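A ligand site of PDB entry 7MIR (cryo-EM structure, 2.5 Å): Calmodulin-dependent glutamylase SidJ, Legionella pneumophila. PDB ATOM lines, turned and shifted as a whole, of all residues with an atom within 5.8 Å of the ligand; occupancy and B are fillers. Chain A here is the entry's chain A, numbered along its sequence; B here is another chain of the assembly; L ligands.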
ATOM      1  N   HIS A 397     -20.420  -2.085  13.917  1.00  0.00           N
ATOM      2  CA  HIS A 397     -20.468  -3.223  13.012  1.00  0.00           C
ATOM      3  C   HIS A 397     -19.529  -4.315  13.477  1.00  0.00           C
ATOM      4  O   HIS A 397     -19.898  -5.495  13.507  1.00  0.00           O
ATOM      5  CB  HIS A 397     -20.112  -2.773  11.593  1.00  0.00           C
ATOM      6  CG  HIS A 397     -19.786  -3.895  10.660  1.00  0.00           C
ATOM      7  ND1 HIS A 397     -20.607  -4.986  10.494  1.00  0.00           N
ATOM      8  CD2 HIS A 397     -18.721  -4.105   9.850  1.00  0.00           C
ATOM      9  CE1 HIS A 397     -20.071  -5.819   9.627  1.00  0.00           C
ATOM     10  NE2 HIS A 397     -18.922  -5.302   9.217  1.00  0.00           N
ATOM     11  N   THR A 398     -18.308  -3.945  13.861  1.00  0.00           N
ATOM     12  CA  THR A 398     -17.331  -4.911  14.335  1.00  0.00           C
ATOM     13  C   THR A 398     -16.306  -4.183  15.196  1.00  0.00           C
ATOM     14  O   THR A 398     -16.171  -2.957  15.135  1.00  0.00           O
ATOM     15  CB  THR A 398     -16.642  -5.626  13.164  1.00  0.00           C
ATOM     16  OG1 THR A 398     -15.673  -6.548  13.677  1.00  0.00           O
ATOM     17  CG2 THR A 398     -15.948  -4.626  12.249  1.00  0.00           C
ATOM     18  N   ARG A 405      -9.703   0.085   9.941  1.00  0.00           N
ATOM     19  CA  ARG A 405     -10.855   0.146   9.058  1.00  0.00           C
ATOM     20  C   ARG A 405     -11.179   1.580   8.702  1.00  0.00           C
ATOM     21  O   ARG A 405     -10.985   2.500   9.494  1.00  0.00           O
ATOM     22  CB  ARG A 405     -12.070  -0.509   9.722  1.00  0.00           C
ATOM     23  CG  ARG A 405     -12.021  -2.027   9.762  1.00  0.00           C
ATOM     24  CD  ARG A 405     -13.268  -2.584  10.424  1.00  0.00           C
ATOM     25  NE  ARG A 405     -14.455  -2.391   9.589  1.00  0.00           N
ATOM     26  CZ  ARG A 405     -14.893  -3.268   8.694  1.00  0.00           C
ATOM     27  NH1 ARG A 405     -14.279  -4.420   8.490  1.00  0.00           N
ATOM     28  NH2 ARG A 405     -15.977  -2.977   7.979  1.00  0.00           N
ATOM     29  N   ASP A 407     -14.207   2.757   8.205  1.00  0.00           N
ATOM     30  CA  ASP A 407     -15.356   3.157   8.991  1.00  0.00           C
ATOM     31  C   ASP A 407     -15.080   3.197  10.482  1.00  0.00           C
ATOM     32  O   ASP A 407     -15.912   3.696  11.245  1.00  0.00           O
ATOM     33  CB  ASP A 407     -16.538   2.213   8.716  1.00  0.00           C
ATOM     34  CG  ASP A 407     -16.170   0.751   8.886  1.00  0.00           C
ATOM     35  OD1 ASP A 407     -15.243   0.453   9.656  1.00  0.00           O
ATOM     36  OD2 ASP A 407     -16.816  -0.103   8.240  1.00  0.00           O
ATOM     37  N   GLY A 409     -15.217   0.813  12.460  1.00  0.00           N
ATOM     38  CA  GLY A 409     -16.119  -0.099  13.101  1.00  0.00           C
ATOM     39  C   GLY A 409     -17.504   0.454  13.367  1.00  0.00           C
ATOM     40  O   GLY A 409     -18.376  -0.300  13.815  1.00  0.00           O
ATOM     41  N   ARG A 410     -17.742   1.733  13.103  1.00  0.00           N
ATOM     42  CA  ARG A 410     -19.046   2.319  13.343  1.00  0.00           C
ATOM     43  C   ARG A 410     -20.047   1.802  12.314  1.00  0.00           C
ATOM     44  O   ARG A 410     -19.761   1.788  11.111  1.00  0.00           O
ATOM     45  CB  ARG A 410     -18.969   3.842  13.274  1.00  0.00           C
ATOM     46  CG  ARG A 410     -20.122   4.552  13.941  1.00  0.00           C
ATOM     47  CD  ARG A 410     -19.877   6.041  14.055  1.00  0.00           C
ATOM     48  NE  ARG A 410     -21.047   6.765  14.515  1.00  0.00           N
ATOM     49  CZ  ARG A 410     -21.967   7.316  13.730  1.00  0.00           C
ATOM     50  NH1 ARG A 410     -21.881   7.233  12.413  1.00  0.00           N
ATOM     51  NH2 ARG A 410     -22.995   7.955  14.281  1.00  0.00           N
ATOM     52  N   TYR A 411     -21.216   1.394  12.794  1.00  0.00           N
ATOM     53  CA  TYR A 411     -22.249   0.870  11.899  1.00  0.00           C
ATOM     54  C   TYR A 411     -22.757   1.965  10.970  1.00  0.00           C
ATOM     55  O   TYR A 411     -23.033   3.083  11.409  1.00  0.00           O
ATOM     56  CB  TYR A 411     -23.408   0.304  12.723  1.00  0.00           C
ATOM     57  CG  TYR A 411     -24.254  -0.689  11.967  1.00  0.00           C
ATOM     58  CD1 TYR A 411     -23.894  -2.020  11.894  1.00  0.00           C
ATOM     59  CD2 TYR A 411     -25.416  -0.287  11.333  1.00  0.00           C
ATOM     60  CE1 TYR A 411     -24.648  -2.926  11.202  1.00  0.00           C
ATOM     61  CE2 TYR A 411     -26.191  -1.189  10.633  1.00  0.00           C
ATOM     62  CZ  TYR A 411     -25.801  -2.514  10.575  1.00  0.00           C
ATOM     63  OH  TYR A 411     -26.558  -3.429   9.898  1.00  0.00           O
ATOM     64  N   GLN A 412     -22.863   1.646   9.684  1.00  0.00           N
ATOM     65  CA  GLN A 412     -23.387   2.557   8.681  1.00  0.00           C
ATOM     66  C   GLN A 412     -24.730   2.043   8.199  1.00  0.00           C
ATOM     67  O   GLN A 412     -24.823   0.923   7.681  1.00  0.00           O
ATOM     68  CB  GLN A 412     -22.418   2.683   7.503  1.00  0.00           C
ATOM     69  CG  GLN A 412     -21.232   3.575   7.782  1.00  0.00           C
ATOM     70  CD  GLN A 412     -20.109   3.405   6.781  1.00  0.00           C
ATOM     71  OE1 GLN A 412     -20.043   2.407   6.073  1.00  0.00           O
ATOM     72  NE2 GLN A 412     -19.234   4.392   6.716  1.00  0.00           N
ATOM     73  N   ALA A 413     -25.774   2.860   8.362  1.00  0.00           N
ATOM     74  CA  ALA A 413     -27.107   2.430   7.961  1.00  0.00           C
ATOM     75  C   ALA A 413     -27.193   2.209   6.458  1.00  0.00           C
ATOM     76  O   ALA A 413     -27.680   1.169   5.996  1.00  0.00           O
ATOM     77  CB  ALA A 413     -28.138   3.463   8.417  1.00  0.00           C
ATOM     78  N   VAL A 415     -24.902   1.512   4.055  1.00  0.00           N
ATOM     79  CA  VAL A 415     -23.534   1.113   3.730  1.00  0.00           C
ATOM     80  C   VAL A 415     -23.333   1.028   2.221  1.00  0.00           C
ATOM     81  O   VAL A 415     -22.270   1.363   1.703  1.00  0.00           O
ATOM     82  CB  VAL A 415     -23.193  -0.227   4.415  1.00  0.00           C
ATOM     83  CG1 VAL A 415     -23.861  -1.396   3.709  1.00  0.00           C
ATOM     84  CG2 VAL A 415     -21.689  -0.420   4.461  1.00  0.00           C
ATOM     85  N   ASN A 419     -19.884   3.441   0.256  1.00  0.00           N
ATOM     86  CA  ASN A 419     -18.695   2.679  -0.066  1.00  0.00           C
ATOM     87  C   ASN A 419     -18.797   2.179  -1.496  1.00  0.00           C
ATOM     88  O   ASN A 419     -19.856   2.224  -2.116  1.00  0.00           O
ATOM     89  CB  ASN A 419     -18.503   1.496   0.899  1.00  0.00           C
ATOM     90  CG  ASN A 419     -18.496   1.924   2.350  1.00  0.00           C
ATOM     91  OD1 ASN A 419     -19.513   1.884   3.022  1.00  0.00           O
ATOM     92  ND2 ASN A 419     -17.330   2.340   2.827  1.00  0.00           N
ATOM     93  N   GLN A 422     -19.956  -2.497  -1.829  1.00  0.00           N
ATOM     94  CA  GLN A 422     -20.633  -3.060  -0.663  1.00  0.00           C
ATOM     95  C   GLN A 422     -22.098  -3.227  -1.025  1.00  0.00           C
ATOM     96  O   GLN A 422     -22.718  -2.305  -1.560  1.00  0.00           O
ATOM     97  CB  GLN A 422     -20.489  -2.159   0.567  1.00  0.00           C
ATOM     98  CG  GLN A 422     -19.057  -1.910   1.007  1.00  0.00           C
ATOM     99  CD  GLN A 422     -18.471  -3.070   1.767  1.00  0.00           C
ATOM    100  OE1 GLN A 422     -19.010  -4.179   1.754  1.00  0.00           O
ATOM    101  NE2 GLN A 422     -17.361  -2.827   2.457  1.00  0.00           N
ATOM    102  N   PHE A 423     -22.659  -4.408  -0.737  1.00  0.00           N
ATOM    103  CA  PHE A 423     -23.941  -4.785  -1.295  1.00  0.00           C
ATOM    104  C   PHE A 423     -25.070  -4.939  -0.288  1.00  0.00           C
ATOM    105  O   PHE A 423     -26.227  -5.068  -0.712  1.00  0.00           O
ATOM    106  CB  PHE A 423     -23.798  -6.088  -2.092  1.00  0.00           C
ATOM    107  CG  PHE A 423     -22.759  -6.011  -3.177  1.00  0.00           C
ATOM    108  CD1 PHE A 423     -22.993  -5.267  -4.330  1.00  0.00           C
ATOM    109  CD2 PHE A 423     -21.541  -6.644  -3.043  1.00  0.00           C
ATOM    110  CE1 PHE A 423     -22.040  -5.189  -5.314  1.00  0.00           C
ATOM    111  CE2 PHE A 423     -20.588  -6.565  -4.027  1.00  0.00           C
ATOM    112  CZ  PHE A 423     -20.839  -5.828  -5.167  1.00  0.00           C
ATOM    113  N   GLN A 424     -24.795  -4.939   1.013  1.00  0.00           N
ATOM    114  CA  GLN A 424     -25.877  -5.094   1.980  1.00  0.00           C
ATOM    115  C   GLN A 424     -25.366  -4.839   3.386  1.00  0.00           C
ATOM    116  O   GLN A 424     -24.165  -4.880   3.645  1.00  0.00           O
ATOM    117  CB  GLN A 424     -26.527  -6.472   1.870  1.00  0.00           C
ATOM    118  CG  GLN A 424     -25.552  -7.606   1.623  1.00  0.00           C
ATOM    119  CD  GLN A 424     -26.246  -8.937   1.451  1.00  0.00           C
ATOM    120  OE1 GLN A 424     -27.448  -9.055   1.677  1.00  0.00           O
ATOM    121  NE2 GLN A 424     -25.484  -9.954   1.056  1.00  0.00           N
ATOM    122  N   LEU A 425     -26.307  -4.587   4.293  1.00  0.00           N
ATOM    123  CA  LEU A 425     -25.969  -4.269   5.670  1.00  0.00           C
ATOM    124  C   LEU A 425     -25.364  -5.465   6.384  1.00  0.00           C
ATOM    125  O   LEU A 425     -25.730  -6.620   6.136  1.00  0.00           O
ATOM    126  CB  LEU A 425     -27.209  -3.791   6.425  1.00  0.00           C
ATOM    127  CG  LEU A 425     -27.527  -2.304   6.335  1.00  0.00           C
ATOM    128  CD1 LEU A 425     -27.596  -1.863   4.884  1.00  0.00           C
ATOM    129  CD2 LEU A 425     -28.816  -1.982   7.061  1.00  0.00           C
ATOM    130  N   GLY A 426     -24.430  -5.186   7.296  1.00  0.00           N
ATOM    131  CA  GLY A 426     -23.676  -6.219   7.980  1.00  0.00           C
ATOM    132  C   GLY A 426     -24.153  -6.472   9.394  1.00  0.00           C
ATOM    133  O   GLY A 426     -25.151  -5.934   9.868  1.00  0.00           O
ATOM    134  N   ARG A 427     -23.382  -7.304  10.088  1.00  0.00           N
ATOM    135  CA  ARG A 427     -23.720  -7.721  11.442  1.00  0.00           C
ATOM    136  C   ARG A 427     -23.623  -6.558  12.426  1.00  0.00           C
ATOM    137  O   ARG A 427     -22.783  -5.670  12.287  1.00  0.00           O
ATOM    138  CB  ARG A 427     -22.780  -8.855  11.874  1.00  0.00           C
ATOM    139  CG  ARG A 427     -22.675  -9.096  13.372  1.00  0.00           C
ATOM    140  CD  ARG A 427     -21.613 -10.139  13.671  1.00  0.00           C
ATOM    141  NE  ARG A 427     -20.281  -9.566  13.665  1.00  0.00           N
ATOM    142  CZ  ARG A 427     -19.566  -9.276  14.741  1.00  0.00           C
ATOM    143  NH1 ARG A 427     -20.028  -9.490  15.961  1.00  0.00           N
ATOM    144  NH2 ARG A 427     -18.348  -8.749  14.590  1.00  0.00           N
ATOM    145  N   ASN A 638     -18.856 -11.937   9.647  1.00  0.00           N
ATOM    146  CA  ASN A 638     -18.582 -11.644   8.240  1.00  0.00           C
ATOM    147  C   ASN A 638     -19.763 -11.907   7.291  1.00  0.00           C
ATOM    148  O   ASN A 638     -19.576 -12.126   6.109  1.00  0.00           O
ATOM    149  CB  ASN A 638     -17.270 -12.286   7.734  1.00  0.00           C
ATOM    150  CG  ASN A 638     -16.895 -11.849   6.324  1.00  0.00           C
ATOM    151  OD1 ASN A 638     -16.512 -10.701   6.106  1.00  0.00           O
ATOM    152  ND2 ASN A 638     -16.997 -12.765   5.374  1.00  0.00           N
ATOM    153  N   ARG A 639     -20.983 -11.883   7.841  1.00  0.00           N
ATOM    154  CA  ARG A 639     -22.175 -12.045   7.020  1.00  0.00           C
ATOM    155  C   ARG A 639     -23.032 -10.798   7.139  1.00  0.00           C
ATOM    156  O   ARG A 639     -22.665  -9.817   7.789  1.00  0.00           O
ATOM    157  CB  ARG A 639     -22.963 -13.296   7.455  1.00  0.00           C
ATOM    158  CG  ARG A 639     -22.207 -14.598   7.283  1.00  0.00           C
ATOM    159  CD  ARG A 639     -21.874 -14.880   5.823  1.00  0.00           C
ATOM    160  NE  ARG A 639     -22.824 -15.794   5.205  1.00  0.00           N
ATOM    161  CZ  ARG A 639     -22.949 -17.071   5.504  1.00  0.00           C
ATOM    162  NH1 ARG A 639     -22.173 -17.649   6.409  1.00  0.00           N
ATOM    163  NH2 ARG A 639     -23.856 -17.811   4.871  1.00  0.00           N
ATOM    164  N   GLU A 640     -24.199 -10.834   6.496  1.00  0.00           N
ATOM    165  CA  GLU A 640     -25.122  -9.712   6.499  1.00  0.00           C
ATOM    166  C   GLU A 640     -26.119  -9.845   7.647  1.00  0.00           C
ATOM    167  O   GLU A 640     -26.311 -10.922   8.213  1.00  0.00           O
ATOM    168  CB  GLU A 640     -25.858  -9.613   5.157  1.00  0.00           C
ATOM    169  CG  GLU A 640     -26.964 -10.630   4.941  1.00  0.00           C
ATOM    170  CD  GLU A 640     -26.442 -12.024   4.654  1.00  0.00           C
ATOM    171  OE1 GLU A 640     -25.214 -12.241   4.763  1.00  0.00           O
ATOM    172  OE2 GLU A 640     -27.254 -12.910   4.320  1.00  0.00           O
ATOM    173  N   ARG B 629      -8.604  -8.657   4.403  1.00  0.00           N
ATOM    174  CA  ARG B 629      -9.124  -7.431   3.806  1.00  0.00           C
ATOM    175  C   ARG B 629      -7.996  -6.679   3.096  1.00  0.00           C
ATOM    176  O   ARG B 629      -6.859  -6.636   3.566  1.00  0.00           O
ATOM    177  CB  ARG B 629      -9.744  -6.540   4.884  1.00  0.00           C
ATOM    178  CG  ARG B 629     -10.911  -5.700   4.400  1.00  0.00           C
ATOM    179  CD  ARG B 629     -11.575  -4.940   5.541  1.00  0.00           C
ATOM    180  NE  ARG B 629     -10.691  -3.933   6.106  1.00  0.00           N
ATOM    181  CZ  ARG B 629      -9.836  -4.144   7.108  1.00  0.00           C
ATOM    182  NH1 ARG B 629      -9.733  -5.330   7.684  1.00  0.00           N
ATOM    183  NH2 ARG B 629      -9.059  -3.155   7.512  1.00  0.00           N
ATOM    184  N   GLU B 635     -13.350  -8.476   1.502  1.00  0.00           N
ATOM    185  CA  GLU B 635     -13.825  -9.232   2.656  1.00  0.00           C
ATOM    186  C   GLU B 635     -14.656 -10.455   2.270  1.00  0.00           C
ATOM    187  O   GLU B 635     -14.866 -11.330   3.114  1.00  0.00           O
ATOM    188  CB  GLU B 635     -14.648  -8.329   3.579  1.00  0.00           C
ATOM    189  CG  GLU B 635     -15.750  -7.522   2.902  1.00  0.00           C
ATOM    190  CD  GLU B 635     -17.048  -8.284   2.737  1.00  0.00           C
ATOM    191  OE1 GLU B 635     -17.180  -9.371   3.329  1.00  0.00           O
ATOM    192  OE2 GLU B 635     -17.934  -7.798   2.007  1.00  0.00           O
HETATM  193  P1  LIG L   1     -16.876  -6.403   6.115  1.00  0.00           P
HETATM  194  O1  LIG L   1     -15.986  -7.591   6.093  1.00  0.00           O
HETATM  195  O2  LIG L   1     -16.371  -5.128   5.449  1.00  0.00           O
HETATM  196  O3  LIG L   1     -17.292  -6.045   7.537  1.00  0.00           O
HETATM  197  O4  LIG L   1     -18.213  -6.799   5.364  1.00  0.00           O
HETATM  198  C1  LIG L   1     -19.123  -7.745   5.914  1.00  0.00           C
HETATM  199  C2  LIG L   1     -20.554  -7.308   5.716  1.00  0.00           C
HETATM  200  O5  LIG L   1     -20.812  -6.133   6.543  1.00  0.00           O
HETATM  201  C3  LIG L   1     -20.930  -6.906   4.299  1.00  0.00           C
HETATM  202  O6  LIG L   1     -22.297  -7.230   4.059  1.00  0.00           O
HETATM  203  C4  LIG L   1     -20.754  -5.399   4.315  1.00  0.00           C
HETATM  204  O7  LIG L   1     -21.517  -4.705   3.346  1.00  0.00           O
HETATM  205  C5  LIG L   1     -21.208  -5.055   5.728  1.00  0.00           C
HETATM  206  N1  LIG L   1     -20.614  -3.838   6.278  1.00  0.00           N
HETATM  207  C6  LIG L   1     -19.320  -3.409   6.116  1.00  0.00           C
HETATM  208  N2  LIG L   1     -19.031  -2.310   6.768  1.00  0.00           N
HETATM  209  C7  LIG L   1     -20.215  -1.993   7.415  1.00  0.00           C
HETATM  210  C8  LIG L   1     -20.573  -0.949   8.287  1.00  0.00           C
HETATM  211  N3  LIG L   1     -19.699  -0.021   8.679  1.00  0.00           N
HETATM  212  N4  LIG L   1     -21.841  -0.910   8.748  1.00  0.00           N
HETATM  213  C9  LIG L   1     -22.693  -1.873   8.359  1.00  0.00           C
HETATM  214  N5  LIG L   1     -22.467  -2.908   7.549  1.00  0.00           N
HETATM  215  C10 LIG L   1     -21.202  -2.915   7.108  1.00  0.00           C
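The side-chain amide oxygen (OE1) of Gln 422 lies within hydrogen-bond range of an oxygen (O7) of the ligand.
The side-chain carboxylate (OD2) of Asp 407 is in hydrogen-bond range of a nitrogen (N3) of the ligand, at 2.9 Å.
The backbone carbonyl oxygen of Arg 410 is in hydrogen-bond range of a nitrogen (N3) of the ligand, at 3.0 Å.
An oxygen (O2) of the ligand lies within salt-bridge range of the guanidinium group (NH2) of Arg 405.
An oxygen (O7) of the ligand lies within hydrogen-bond range of the backbone carbonyl oxygen of Gln 424, at 2.7 Å.
A ring nitrogen (NE2) of His 397 lies within hydrogen-bond range of an oxygen (O3) of the ligand (2.5 Å).
The backbone NH (N) of Gln 412 is in hydrogen-bond range of a nitrogen (N4) of the ligand, at 2.9 Å.
OD1 of Asn 638 lies close to O1 of the ligand (3.2 Å).
The backbone NH of Gly 426 is in hydrogen-bond range of a nitrogen (N5) of the ligand, at 3.0 Å.
The side-chain carboxylate of Glu 635 of chain B sits close to an oxygen (O4) of the ligand.
Merely in contact with the ligand: Tyr 411 (3.6 Å), Val 415 (3.7 Å) and Arg 639 (3.9 Å).
Hydrophobic or aromatic side chains that line the ligand: His 397, Tyr 411 and Val 415.
13 residues have an atom within 4 Å of the ligand: His 397, Arg 405, Asp 407, Arg 410, Tyr 411, Gln 412, Val 415, Gln 422, Gln 424, Gly 426, Asn 638, Arg 639 and Glu 635 of chain B.
The nearest printed residue that does not touch the ligand is Leu 425 (4.04 Å).
The side-chain carboxylate (OD1) of Asp 407 is in hydrogen-bond range of the backbone NH (N) of Gly 409 (2.8 Å).
The side-chain amide oxygen (OD1) of Asn 419 lies close to the backbone carbonyl oxygen (O) of Val 415.
The side-chain carboxylate (OD1) of Asp 407 lies within salt-bridge range of the guanidinium group (NE) of Arg 405 (3.0 Å).
OE1 of Gln 412 sits close to OD1 of Asn 419, at 3.1 Å.
O of Arg 427 sits at hydrogen-bond distance from ND1 of His 397 (2.9 Å).
The side-chain carboxylate (OE1) of Glu 635 of chain B sits close to the side-chain amide oxygen (OD1) of Asn 638 (3.2 Å).
OH of Tyr 411 is in hydrogen-bond range of O of Gly 426 (2.9 Å).
The backbone carbonyl oxygen (O) of Gly 409 lies within hydrogen-bond range of the backbone NH (N) of His 397 (2.7 Å).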
